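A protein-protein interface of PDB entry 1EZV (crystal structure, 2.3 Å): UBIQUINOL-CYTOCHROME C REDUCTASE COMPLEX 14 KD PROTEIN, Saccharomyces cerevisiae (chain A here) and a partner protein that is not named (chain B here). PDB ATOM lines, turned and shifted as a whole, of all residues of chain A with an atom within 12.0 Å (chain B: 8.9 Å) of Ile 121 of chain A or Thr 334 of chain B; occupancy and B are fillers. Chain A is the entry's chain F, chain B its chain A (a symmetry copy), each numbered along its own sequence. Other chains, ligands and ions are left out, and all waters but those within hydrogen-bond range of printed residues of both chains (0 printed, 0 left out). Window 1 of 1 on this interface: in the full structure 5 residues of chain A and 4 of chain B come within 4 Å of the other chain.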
ATOM      1  N   ALA A 111     -19.236  45.177 -11.115  1.00  0.00           N
ATOM      2  CA  ALA A 111     -20.455  44.387 -11.306  1.00  0.00           C
ATOM      3  C   ALA A 111     -20.125  42.948 -11.704  1.00  0.00           C
ATOM      4  O   ALA A 111     -20.620  42.003 -11.092  1.00  0.00           O
ATOM      5  CB  ALA A 111     -21.342  45.029 -12.354  1.00  0.00           C
ATOM      6  N   ALA A 112     -19.181  42.798 -12.630  1.00  0.00           N
ATOM      7  CA  ALA A 112     -18.742  41.486 -13.097  1.00  0.00           C
ATOM      8  C   ALA A 112     -18.056  40.679 -11.996  1.00  0.00           C
ATOM      9  O   ALA A 112     -18.317  39.486 -11.838  1.00  0.00           O
ATOM     10  CB  ALA A 112     -17.809  41.644 -14.299  1.00  0.00           C
ATOM     11  N   LYS A 113     -17.180  41.332 -11.239  1.00  0.00           N
ATOM     12  CA  LYS A 113     -16.479  40.676 -10.140  1.00  0.00           C
ATOM     13  C   LYS A 113     -17.442  40.177  -9.054  1.00  0.00           C
ATOM     14  O   LYS A 113     -17.313  39.050  -8.577  1.00  0.00           O
ATOM     15  CB  LYS A 113     -15.444  41.631  -9.535  1.00  0.00           C
ATOM     16  CG  LYS A 113     -14.586  41.010  -8.438  1.00  0.00           C
ATOM     17  CD  LYS A 113     -13.913  39.719  -8.911  1.00  0.00           C
ATOM     18  CE  LYS A 113     -12.413  39.914  -9.149  1.00  0.00           C
ATOM     19  NZ  LYS A 113     -11.670  40.242  -7.894  1.00  0.00           N
ATOM     20  N   GLU A 114     -18.465  40.971  -8.750  1.00  0.00           N
ATOM     21  CA  GLU A 114     -19.484  40.556  -7.788  1.00  0.00           C
ATOM     22  C   GLU A 114     -20.272  39.324  -8.258  1.00  0.00           C
ATOM     23  O   GLU A 114     -20.497  38.387  -7.477  1.00  0.00           O
ATOM     24  CB  GLU A 114     -20.445  41.712  -7.490  1.00  0.00           C
ATOM     25  CG  GLU A 114     -21.477  41.390  -6.417  1.00  0.00           C
ATOM     26  CD  GLU A 114     -22.353  42.579  -6.057  1.00  0.00           C
ATOM     27  OE1 GLU A 114     -22.943  43.195  -6.971  1.00  0.00           O
ATOM     28  OE2 GLU A 114     -22.467  42.885  -4.850  1.00  0.00           O
ATOM     29  N   LYS A 115     -20.651  39.302  -9.538  1.00  0.00           N
ATOM     30  CA  LYS A 115     -21.365  38.151 -10.085  1.00  0.00           C
ATOM     31  C   LYS A 115     -20.523  36.890  -9.980  1.00  0.00           C
ATOM     32  O   LYS A 115     -21.005  35.842  -9.548  1.00  0.00           O
ATOM     33  CB  LYS A 115     -21.753  38.383 -11.544  1.00  0.00           C
ATOM     34  CG  LYS A 115     -22.669  37.296 -12.094  1.00  0.00           C
ATOM     35  CD  LYS A 115     -22.676  37.277 -13.616  1.00  0.00           C
ATOM     36  CE  LYS A 115     -23.777  36.374 -14.153  1.00  0.00           C
ATOM     37  NZ  LYS A 115     -23.717  35.005 -13.567  1.00  0.00           N
ATOM     38  N   ASP A 116     -19.236  37.027 -10.267  1.00  0.00           N
ATOM     39  CA  ASP A 116     -18.331  35.895 -10.185  1.00  0.00           C
ATOM     40  C   ASP A 116     -18.194  35.428  -8.731  1.00  0.00           C
ATOM     41  O   ASP A 116     -18.179  34.226  -8.455  1.00  0.00           O
ATOM     42  CB  ASP A 116     -16.969  36.282 -10.766  1.00  0.00           C
ATOM     43  CG  ASP A 116     -16.044  35.090 -10.930  1.00  0.00           C
ATOM     44  OD1 ASP A 116     -16.276  34.278 -11.856  1.00  0.00           O
ATOM     45  OD2 ASP A 116     -15.099  34.955 -10.120  1.00  0.00           O
ATOM     46  N   GLU A 117     -18.223  36.386  -7.805  1.00  0.00           N
ATOM     47  CA  GLU A 117     -18.148  36.095  -6.374  1.00  0.00           C
ATOM     48  C   GLU A 117     -19.409  35.392  -5.890  1.00  0.00           C
ATOM     49  O   GLU A 117     -19.335  34.345  -5.239  1.00  0.00           O
ATOM     50  CB  GLU A 117     -17.939  37.389  -5.585  1.00  0.00           C
ATOM     51  CG  GLU A 117     -16.569  37.504  -4.932  1.00  0.00           C
ATOM     52  CD  GLU A 117     -16.009  38.918  -4.956  1.00  0.00           C
ATOM     53  OE1 GLU A 117     -16.788  39.892  -4.821  1.00  0.00           O
ATOM     54  OE2 GLU A 117     -14.776  39.055  -5.121  1.00  0.00           O
ATOM     55  N   LEU A 118     -20.563  35.923  -6.286  1.00  0.00           N
ATOM     56  CA  LEU A 118     -21.840  35.352  -5.883  1.00  0.00           C
ATOM     57  C   LEU A 118     -22.164  33.999  -6.533  1.00  0.00           C
ATOM     58  O   LEU A 118     -22.771  33.141  -5.891  1.00  0.00           O
ATOM     59  CB  LEU A 118     -22.966  36.356  -6.142  1.00  0.00           C
ATOM     60  CG  LEU A 118     -22.879  37.640  -5.302  1.00  0.00           C
ATOM     61  CD1 LEU A 118     -23.874  38.661  -5.812  1.00  0.00           C
ATOM     62  CD2 LEU A 118     -23.137  37.327  -3.832  1.00  0.00           C
ATOM     63  N   ASP A 119     -21.721  33.778  -7.775  1.00  0.00           N
ATOM     64  CA  ASP A 119     -21.905  32.474  -8.431  1.00  0.00           C
ATOM     65  C   ASP A 119     -21.081  31.380  -7.735  1.00  0.00           C
ATOM     66  O   ASP A 119     -21.340  30.189  -7.908  1.00  0.00           O
ATOM     67  CB  ASP A 119     -21.493  32.529  -9.915  1.00  0.00           C
ATOM     68  CG  ASP A 119     -22.431  33.371 -10.770  1.00  0.00           C
ATOM     69  OD1 ASP A 119     -23.578  33.629 -10.357  1.00  0.00           O
ATOM     70  OD2 ASP A 119     -22.016  33.765 -11.881  1.00  0.00           O
ATOM     71  N   ASN A 120     -20.086  31.786  -6.954  1.00  0.00           N
ATOM     72  CA  ASN A 120     -19.171  30.826  -6.359  1.00  0.00           C
ATOM     73  C   ASN A 120     -19.132  30.857  -4.832  1.00  0.00           C
ATOM     74  O   ASN A 120     -18.270  30.216  -4.230  1.00  0.00           O
ATOM     75  CB  ASN A 120     -17.759  31.032  -6.920  1.00  0.00           C
ATOM     76  CG  ASN A 120     -17.663  30.700  -8.401  1.00  0.00           C
ATOM     77  OD1 ASN A 120     -17.939  29.578  -8.816  1.00  0.00           O
ATOM     78  ND2 ASN A 120     -17.311  31.694  -9.208  1.00  0.00           N
ATOM     79  N   ILE A 121     -20.085  31.550  -4.205  1.00  0.00           N
ATOM     80  CA  ILE A 121     -20.129  31.621  -2.739  1.00  0.00           C
ATOM     81  C   ILE A 121     -20.299  30.251  -2.095  1.00  0.00           C
ATOM     82  O   ILE A 121     -21.156  29.474  -2.503  1.00  0.00           O
ATOM     83  CB  ILE A 121     -21.277  32.530  -2.212  1.00  0.00           C
ATOM     84  CG1 ILE A 121     -22.575  32.235  -2.959  1.00  0.00           C
ATOM     85  CG2 ILE A 121     -20.883  33.994  -2.312  1.00  0.00           C
ATOM     86  CD1 ILE A 121     -23.710  33.167  -2.603  1.00  0.00           C
ATOM     87  N   GLU A 122     -19.455  29.954  -1.110  1.00  0.00           N
ATOM     88  CA  GLU A 122     -19.637  28.775  -0.270  1.00  0.00           C
ATOM     89  C   GLU A 122     -20.550  29.103   0.906  1.00  0.00           C
ATOM     90  O   GLU A 122     -20.830  30.270   1.181  1.00  0.00           O
ATOM     91  CB  GLU A 122     -18.288  28.272   0.243  1.00  0.00           C
ATOM     92  CG  GLU A 122     -17.439  27.586  -0.817  1.00  0.00           C
ATOM     93  CD  GLU A 122     -16.142  27.018  -0.257  1.00  0.00           C
ATOM     94  OE1 GLU A 122     -15.061  27.561  -0.581  1.00  0.00           O
ATOM     95  OE2 GLU A 122     -16.205  26.025   0.505  1.00  0.00           O
ATOM     96  N   VAL A 123     -21.073  28.064   1.549  1.00  0.00           N
ATOM     97  CA  VAL A 123     -21.950  28.235   2.703  1.00  0.00           C
ATOM     98  C   VAL A 123     -21.457  27.413   3.887  1.00  0.00           C
ATOM     99  O   VAL A 123     -20.959  26.297   3.718  1.00  0.00           O
ATOM    100  CB  VAL A 123     -23.407  27.825   2.374  1.00  0.00           C
ATOM    101  CG1 VAL A 123     -24.072  28.902   1.533  1.00  0.00           C
ATOM    102  CG2 VAL A 123     -23.432  26.489   1.640  1.00  0.00           C
ATOM    103  N   SER A 124     -21.544  27.997   5.081  1.00  0.00           N
ATOM    104  CA  SER A 124     -21.141  27.304   6.301  1.00  0.00           C
ATOM    105  C   SER A 124     -22.280  27.219   7.312  1.00  0.00           C
ATOM    106  O   SER A 124     -22.966  28.209   7.581  1.00  0.00           O
ATOM    107  CB  SER A 124     -19.935  27.999   6.935  1.00  0.00           C
ATOM    108  OG  SER A 124     -19.275  27.131   7.841  1.00  0.00           O
ATOM    109  N   LYS A 125     -22.506  26.011   7.823  1.00  0.00           N
ATOM    110  CA  LYS A 125     -23.522  25.768   8.847  1.00  0.00           C
ATOM    111  C   LYS A 125     -22.878  25.479  10.202  1.00  0.00           C
ATOM    112  O   LYS A 125     -23.537  25.752  11.231  1.00  0.00           O
ATOM    113  CB  LYS A 125     -24.420  24.589   8.449  1.00  0.00           C
ATOM    114  CG  LYS A 125     -25.310  24.843   7.234  1.00  0.00           C
ATOM    115  CD  LYS A 125     -24.676  24.322   5.945  1.00  0.00           C
ATOM    116  CE  LYS A 125     -24.569  22.798   5.935  1.00  0.00           C
ATOM    117  NZ  LYS A 125     -25.905  22.129   5.955  1.00  0.00           N
ATOM    118  OXT LYS A 125     -21.736  24.964  10.219  1.00  0.00           O
ATOM    119  N   LEU B 253     -37.104  19.299  -4.308  1.00  0.00           N
ATOM    120  CA  LEU B 253     -35.949  20.172  -4.098  1.00  0.00           C
ATOM    121  C   LEU B 253     -35.156  20.305  -5.403  1.00  0.00           C
ATOM    122  O   LEU B 253     -34.815  21.414  -5.820  1.00  0.00           O
ATOM    123  CB  LEU B 253     -35.052  19.612  -2.980  1.00  0.00           C
ATOM    124  CG  LEU B 253     -33.817  20.433  -2.577  1.00  0.00           C
ATOM    125  CD1 LEU B 253     -33.530  20.252  -1.105  1.00  0.00           C
ATOM    126  CD2 LEU B 253     -32.600  20.010  -3.392  1.00  0.00           C
ATOM    127  N   ILE B 257     -34.011  23.743  -7.661  1.00  0.00           N
ATOM    128  CA  ILE B 257     -32.666  24.118  -8.082  1.00  0.00           C
ATOM    129  C   ILE B 257     -32.697  24.867  -9.419  1.00  0.00           C
ATOM    130  O   ILE B 257     -32.074  25.923  -9.558  1.00  0.00           O
ATOM    131  CB  ILE B 257     -31.751  22.880  -8.196  1.00  0.00           C
ATOM    132  CG1 ILE B 257     -31.556  22.254  -6.813  1.00  0.00           C
ATOM    133  CG2 ILE B 257     -30.389  23.273  -8.794  1.00  0.00           C
ATOM    134  CD1 ILE B 257     -30.489  21.178  -6.757  1.00  0.00           C
ATOM    135  N   GLY B 272     -30.081  32.822  -8.630  1.00  0.00           N
ATOM    136  CA  GLY B 272     -28.896  31.987  -8.522  1.00  0.00           C
ATOM    137  C   GLY B 272     -29.086  30.653  -9.213  1.00  0.00           C
ATOM    138  O   GLY B 272     -29.049  29.590  -8.575  1.00  0.00           O
ATOM    139  N   LYS B 274     -27.644  28.513 -12.522  1.00  0.00           N
ATOM    140  CA  LYS B 274     -26.559  28.450 -13.506  1.00  0.00           C
ATOM    141  C   LYS B 274     -27.055  28.378 -14.946  1.00  0.00           C
ATOM    142  O   LYS B 274     -26.461  28.986 -15.843  1.00  0.00           O
ATOM    143  CB  LYS B 274     -25.639  27.261 -13.214  1.00  0.00           C
ATOM    144  CG  LYS B 274     -24.756  27.488 -12.011  1.00  0.00           C
ATOM    145  CD  LYS B 274     -23.720  26.397 -11.836  1.00  0.00           C
ATOM    146  CE  LYS B 274     -23.053  26.481 -10.452  1.00  0.00           C
ATOM    147  NZ  LYS B 274     -22.626  27.871 -10.072  1.00  0.00           N
ATOM    148  N   ARG B 326     -26.009  17.587 -14.309  1.00  0.00           N
ATOM    149  CA  ARG B 326     -25.168  17.974 -13.190  1.00  0.00           C
ATOM    150  C   ARG B 326     -25.634  17.389 -11.858  1.00  0.00           C
ATOM    151  O   ARG B 326     -24.804  16.982 -11.046  1.00  0.00           O
ATOM    152  CB  ARG B 326     -25.083  19.496 -13.110  1.00  0.00           C
ATOM    153  CG  ARG B 326     -24.388  20.119 -14.311  1.00  0.00           C
ATOM    154  CD  ARG B 326     -24.233  21.625 -14.143  1.00  0.00           C
ATOM    155  NE  ARG B 326     -23.502  21.930 -12.917  1.00  0.00           N
ATOM    156  CZ  ARG B 326     -24.029  22.532 -11.854  1.00  0.00           C
ATOM    157  NH1 ARG B 326     -23.329  22.613 -10.732  1.00  0.00           N
ATOM    158  NH2 ARG B 326     -25.205  23.135 -11.940  1.00  0.00           N
ATOM    159  N   SER B 330     -22.254  16.704 -10.233  1.00  0.00           N
ATOM    160  CA  SER B 330     -21.539  17.913  -9.827  1.00  0.00           C
ATOM    161  C   SER B 330     -22.366  19.022  -9.169  1.00  0.00           C
ATOM    162  O   SER B 330     -21.888  20.152  -9.041  1.00  0.00           O
ATOM    163  CB  SER B 330     -20.791  18.501 -11.033  1.00  0.00           C
ATOM    164  OG  SER B 330     -21.681  19.194 -11.902  1.00  0.00           O
ATOM    165  N   VAL B 331     -23.596  18.728  -8.758  1.00  0.00           N
ATOM    166  CA  VAL B 331     -24.395  19.741  -8.062  1.00  0.00           C
ATOM    167  C   VAL B 331     -23.691  20.158  -6.752  1.00  0.00           C
ATOM    168  O   VAL B 331     -23.025  19.334  -6.102  1.00  0.00           O
ATOM    169  CB  VAL B 331     -25.854  19.231  -7.789  1.00  0.00           C
ATOM    170  CG1 VAL B 331     -25.846  17.969  -6.933  1.00  0.00           C
ATOM    171  CG2 VAL B 331     -26.679  20.316  -7.132  1.00  0.00           C
ATOM    172  N   THR B 332     -23.656  21.466  -6.498  1.00  0.00           N
ATOM    173  CA  THR B 332     -22.894  22.010  -5.375  1.00  0.00           C
ATOM    174  C   THR B 332     -23.735  22.164  -4.105  1.00  0.00           C
ATOM    175  O   THR B 332     -24.958  22.313  -4.178  1.00  0.00           O
ATOM    176  CB  THR B 332     -22.290  23.392  -5.712  1.00  0.00           C
ATOM    177  OG1 THR B 332     -23.340  24.347  -5.897  1.00  0.00           O
ATOM    178  CG2 THR B 332     -21.449  23.320  -6.976  1.00  0.00           C
ATOM    179  N   ASP B 333     -23.053  22.217  -2.957  1.00  0.00           N
ATOM    180  CA  ASP B 333     -23.683  22.465  -1.654  1.00  0.00           C
ATOM    181  C   ASP B 333     -24.584  23.684  -1.671  1.00  0.00           C
ATOM    182  O   ASP B 333     -25.724  23.632  -1.216  1.00  0.00           O
ATOM    183  CB  ASP B 333     -22.623  22.680  -0.571  1.00  0.00           C
ATOM    184  CG  ASP B 333     -21.984  21.391  -0.110  1.00  0.00           C
ATOM    185  OD1 ASP B 333     -20.738  21.297  -0.172  1.00  0.00           O
ATOM    186  OD2 ASP B 333     -22.719  20.488   0.350  1.00  0.00           O
ATOM    187  N   THR B 334     -24.071  24.789  -2.191  1.00  0.00           N
ATOM    188  CA  THR B 334     -24.805  26.039  -2.116  1.00  0.00           C
ATOM    189  C   THR B 334     -26.018  26.103  -3.052  1.00  0.00           C
ATOM    190  O   THR B 334     -26.996  26.791  -2.742  1.00  0.00           O
ATOM    191  CB  THR B 334     -23.853  27.268  -2.295  1.00  0.00           C
ATOM    192  OG1 THR B 334     -24.406  28.200  -3.234  1.00  0.00           O
ATOM    193  CG2 THR B 334     -22.481  26.819  -2.733  1.00  0.00           C
ATOM    194  N   GLU B 335     -26.024  25.270  -4.096  1.00  0.00           N
ATOM    195  CA  GLU B 335     -27.218  25.108  -4.932  1.00  0.00           C
ATOM    196  C   GLU B 335     -28.319  24.382  -4.158  1.00  0.00           C
ATOM    197  O   GLU B 335     -29.482  24.787  -4.184  1.00  0.00           O
ATOM    198  CB  GLU B 335     -26.895  24.320  -6.206  1.00  0.00           C
ATOM    199  CG  GLU B 335     -26.286  25.139  -7.343  1.00  0.00           C
ATOM    200  CD  GLU B 335     -25.755  24.256  -8.466  1.00  0.00           C
ATOM    201  OE1 GLU B 335     -24.903  23.385  -8.188  1.00  0.00           O
ATOM    202  OE2 GLU B 335     -26.226  24.396  -9.615  1.00  0.00           O
ATOM    203  N   VAL B 336     -27.941  23.288  -3.498  1.00  0.00           N
ATOM    204  CA  VAL B 336     -28.851  22.554  -2.623  1.00  0.00           C
ATOM    205  C   VAL B 336     -29.425  23.444  -1.517  1.00  0.00           C
ATOM    206  O   VAL B 336     -30.644  23.483  -1.317  1.00  0.00           O
ATOM    207  CB  VAL B 336     -28.146  21.344  -1.976  1.00  0.00           C
ATOM    208  CG1 VAL B 336     -29.067  20.678  -0.958  1.00  0.00           C
ATOM    209  CG2 VAL B 336     -27.738  20.354  -3.050  1.00  0.00           C
ATOM    210  N   GLU B 337     -28.548  24.193  -0.848  1.00  0.00           N
ATOM    211  CA  GLU B 337     -28.951  25.102   0.218  1.00  0.00           C
ATOM    212  C   GLU B 337     -29.878  26.204  -0.274  1.00  0.00           C
ATOM    213  O   GLU B 337     -30.850  26.537   0.403  1.00  0.00           O
ATOM    214  CB  GLU B 337     -27.725  25.726   0.895  1.00  0.00           C
ATOM    215  CG  GLU B 337     -26.864  24.744   1.699  1.00  0.00           C
ATOM    216  CD  GLU B 337     -27.633  24.032   2.802  1.00  0.00           C
ATOM    217  OE1 GLU B 337     -27.532  22.786   2.889  1.00  0.00           O
ATOM    218  OE2 GLU B 337     -28.334  24.717   3.581  1.00  0.00           O
ATOM    219  N   ARG B 338     -29.611  26.749  -1.460  1.00  0.00           N
ATOM    220  CA  ARG B 338     -30.501  27.764  -2.024  1.00  0.00           C
ATOM    221  C   ARG B 338     -31.886  27.166  -2.252  1.00  0.00           C
ATOM    222  O   ARG B 338     -32.900  27.815  -1.998  1.00  0.00           O
ATOM    223  CB  ARG B 338     -29.961  28.320  -3.350  1.00  0.00           C
ATOM    224  CG  ARG B 338     -30.692  29.584  -3.815  1.00  0.00           C
ATOM    225  CD  ARG B 338     -30.458  29.918  -5.296  1.00  0.00           C
ATOM    226  NE  ARG B 338     -31.271  29.064  -6.152  1.00  0.00           N
ATOM    227  CZ  ARG B 338     -32.339  29.460  -6.837  1.00  0.00           C
ATOM    228  NH1 ARG B 338     -33.112  28.551  -7.397  1.00  0.00           N
ATOM    229  NH2 ARG B 338     -32.579  30.748  -7.055  1.00  0.00           N
ATOM    230  N   ALA B 339     -31.917  25.896  -2.645  1.00  0.00           N
ATOM    231  CA  ALA B 339     -33.167  25.235  -2.996  1.00  0.00           C
ATOM    232  C   ALA B 339     -33.993  24.936  -1.751  1.00  0.00           C
ATOM    233  O   ALA B 339     -35.203  25.159  -1.739  1.00  0.00           O
ATOM    234  CB  ALA B 339     -32.886  23.955  -3.767  1.00  0.00           C
ATOM    235  N   LYS B 340     -33.325  24.470  -0.698  1.00  0.00           N
ATOM    236  CA  LYS B 340     -33.952  24.289   0.611  1.00  0.00           C
ATOM    237  C   LYS B 340     -34.731  25.532   1.050  1.00  0.00           C
ATOM    238  O   LYS B 340     -35.939  25.467   1.309  1.00  0.00           O
ATOM    239  CB  LYS B 340     -32.893  23.964   1.661  1.00  0.00           C
ATOM    240  CG  LYS B 340     -32.529  22.500   1.740  1.00  0.00           C
ATOM    241  CD  LYS B 340     -31.365  22.294   2.694  1.00  0.00           C
ATOM    242  CE  LYS B 340     -30.807  20.892   2.596  1.00  0.00           C
ATOM    243  NZ  LYS B 340     -29.644  20.723   3.504  1.00  0.00           N
ATOM    244  N   SER B 341     -34.054  26.673   1.058  1.00  0.00           N
ATOM    245  CA  SER B 341     -34.676  27.909   1.504  1.00  0.00           C
ATOM    246  C   SER B 341     -35.877  28.294   0.649  1.00  0.00           C
ATOM    247  O   SER B 341     -36.927  28.672   1.175  1.00  0.00           O
ATOM    248  CB  SER B 341     -33.650  29.037   1.513  1.00  0.00           C
ATOM    249  OG  SER B 341     -32.546  28.681   2.326  1.00  0.00           O
ATOM    250  N   LEU B 342     -35.753  28.117  -0.665  1.00  0.00           N
ATOM    251  CA  LEU B 342     -36.815  28.525  -1.576  1.00  0.00           C
ATOM    252  C   LEU B 342     -37.955  27.508  -1.634  1.00  0.00           C
ATOM    253  O   LEU B 342     -39.103  27.874  -1.905  1.00  0.00           O
ATOM    254  CB  LEU B 342     -36.250  28.766  -2.972  1.00  0.00           C
ATOM    255  CG  LEU B 342     -35.319  29.966  -3.121  1.00  0.00           C
ATOM    256  CD1 LEU B 342     -34.698  29.935  -4.505  1.00  0.00           C
ATOM    257  CD2 LEU B 342     -36.087  31.262  -2.906  1.00  0.00           C
ATOM    258  N   VAL B 388     -26.318  16.807  -0.524  1.00  0.00           N
ATOM    259  CA  VAL B 388     -25.887  16.668  -1.913  1.00  0.00           C
ATOM    260  C   VAL B 388     -25.887  15.197  -2.317  1.00  0.00           C
ATOM    261  O   VAL B 388     -26.370  14.845  -3.396  1.00  0.00           O
ATOM    262  CB  VAL B 388     -24.465  17.264  -2.131  1.00  0.00           C
ATOM    263  CG1 VAL B 388     -23.880  16.789  -3.454  1.00  0.00           C
ATOM    264  CG2 VAL B 388     -24.528  18.781  -2.118  1.00  0.00           C
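Ala 112 of chain A touches none of the printed residues of chain B.
Of the printed residues of chain B, Asp 119 of chain A touches Lys 274.
Of chain B, only Thr 334 comes within 4 Å of Ile 121 of chain A.
Of the printed residues of chain B, Val 123 of chain A touches Glu 337 (3.9 Å).
No residue of chain A comes within 4 Å of Thr 332 of chain B.
Thr 334 of chain B touches one residue of chain A.
No residue of chain A comes within 4 Å of Val 336 of chain B.
Glu 337 of chain B touches just these residues of chain A: Val 123 (3.9 Å) and Lys 125 (3.5 Å).
The nearest residue of chain A that does not touch Thr 334 of chain B is Val 123 of chain A (4.02 Å).
O of Asp 119 of chain A is in hydrogen-bond range of NZ of Lys 274 of chain B, at 3.4 Å.
NZ of Lys 125 of chain A lies within salt-bridge range of OE1 of Glu 337 of chain B (3.5 Å).
The backbone carbonyl oxygen (O) of Glu 337 of chain B is in hydrogen-bond range of the side-chain hydroxyl (OG) of Ser 341 of chain B (3.3 Å).
The side-chain carboxylate (OD2) of Asp 119 of chain A lies within salt-bridge range of the side-chain amino group (NZ) of Lys 115 of chain A.
NZ of Lys 340 of chain B is in salt-bridge range of OE1 of Glu 337 of chain B.
Hydrophobic or aromatic side chains of chain A that line the printed part of chain B: Val 123.
Of the 19 printed residues of chain B, 3 touch a printed residue of chain A.
Along chain B the printed residues that touch a printed residue of chain A span positions 274 to 337.
Among the printed residues, Asp or Glu carboxylates within 4 Å of a Lys or Arg side-chain nitrogen of the other chain: Lys 125 of chain A with Glu 337 of chain B (3.5 Å).
O of Ile 121 of chain A touches CG2 of Thr 334 of chain B (3.0 Å).
Val 123 of chain A touches Glu 337 of chain B (CG2 to CG, 3.9 Å).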
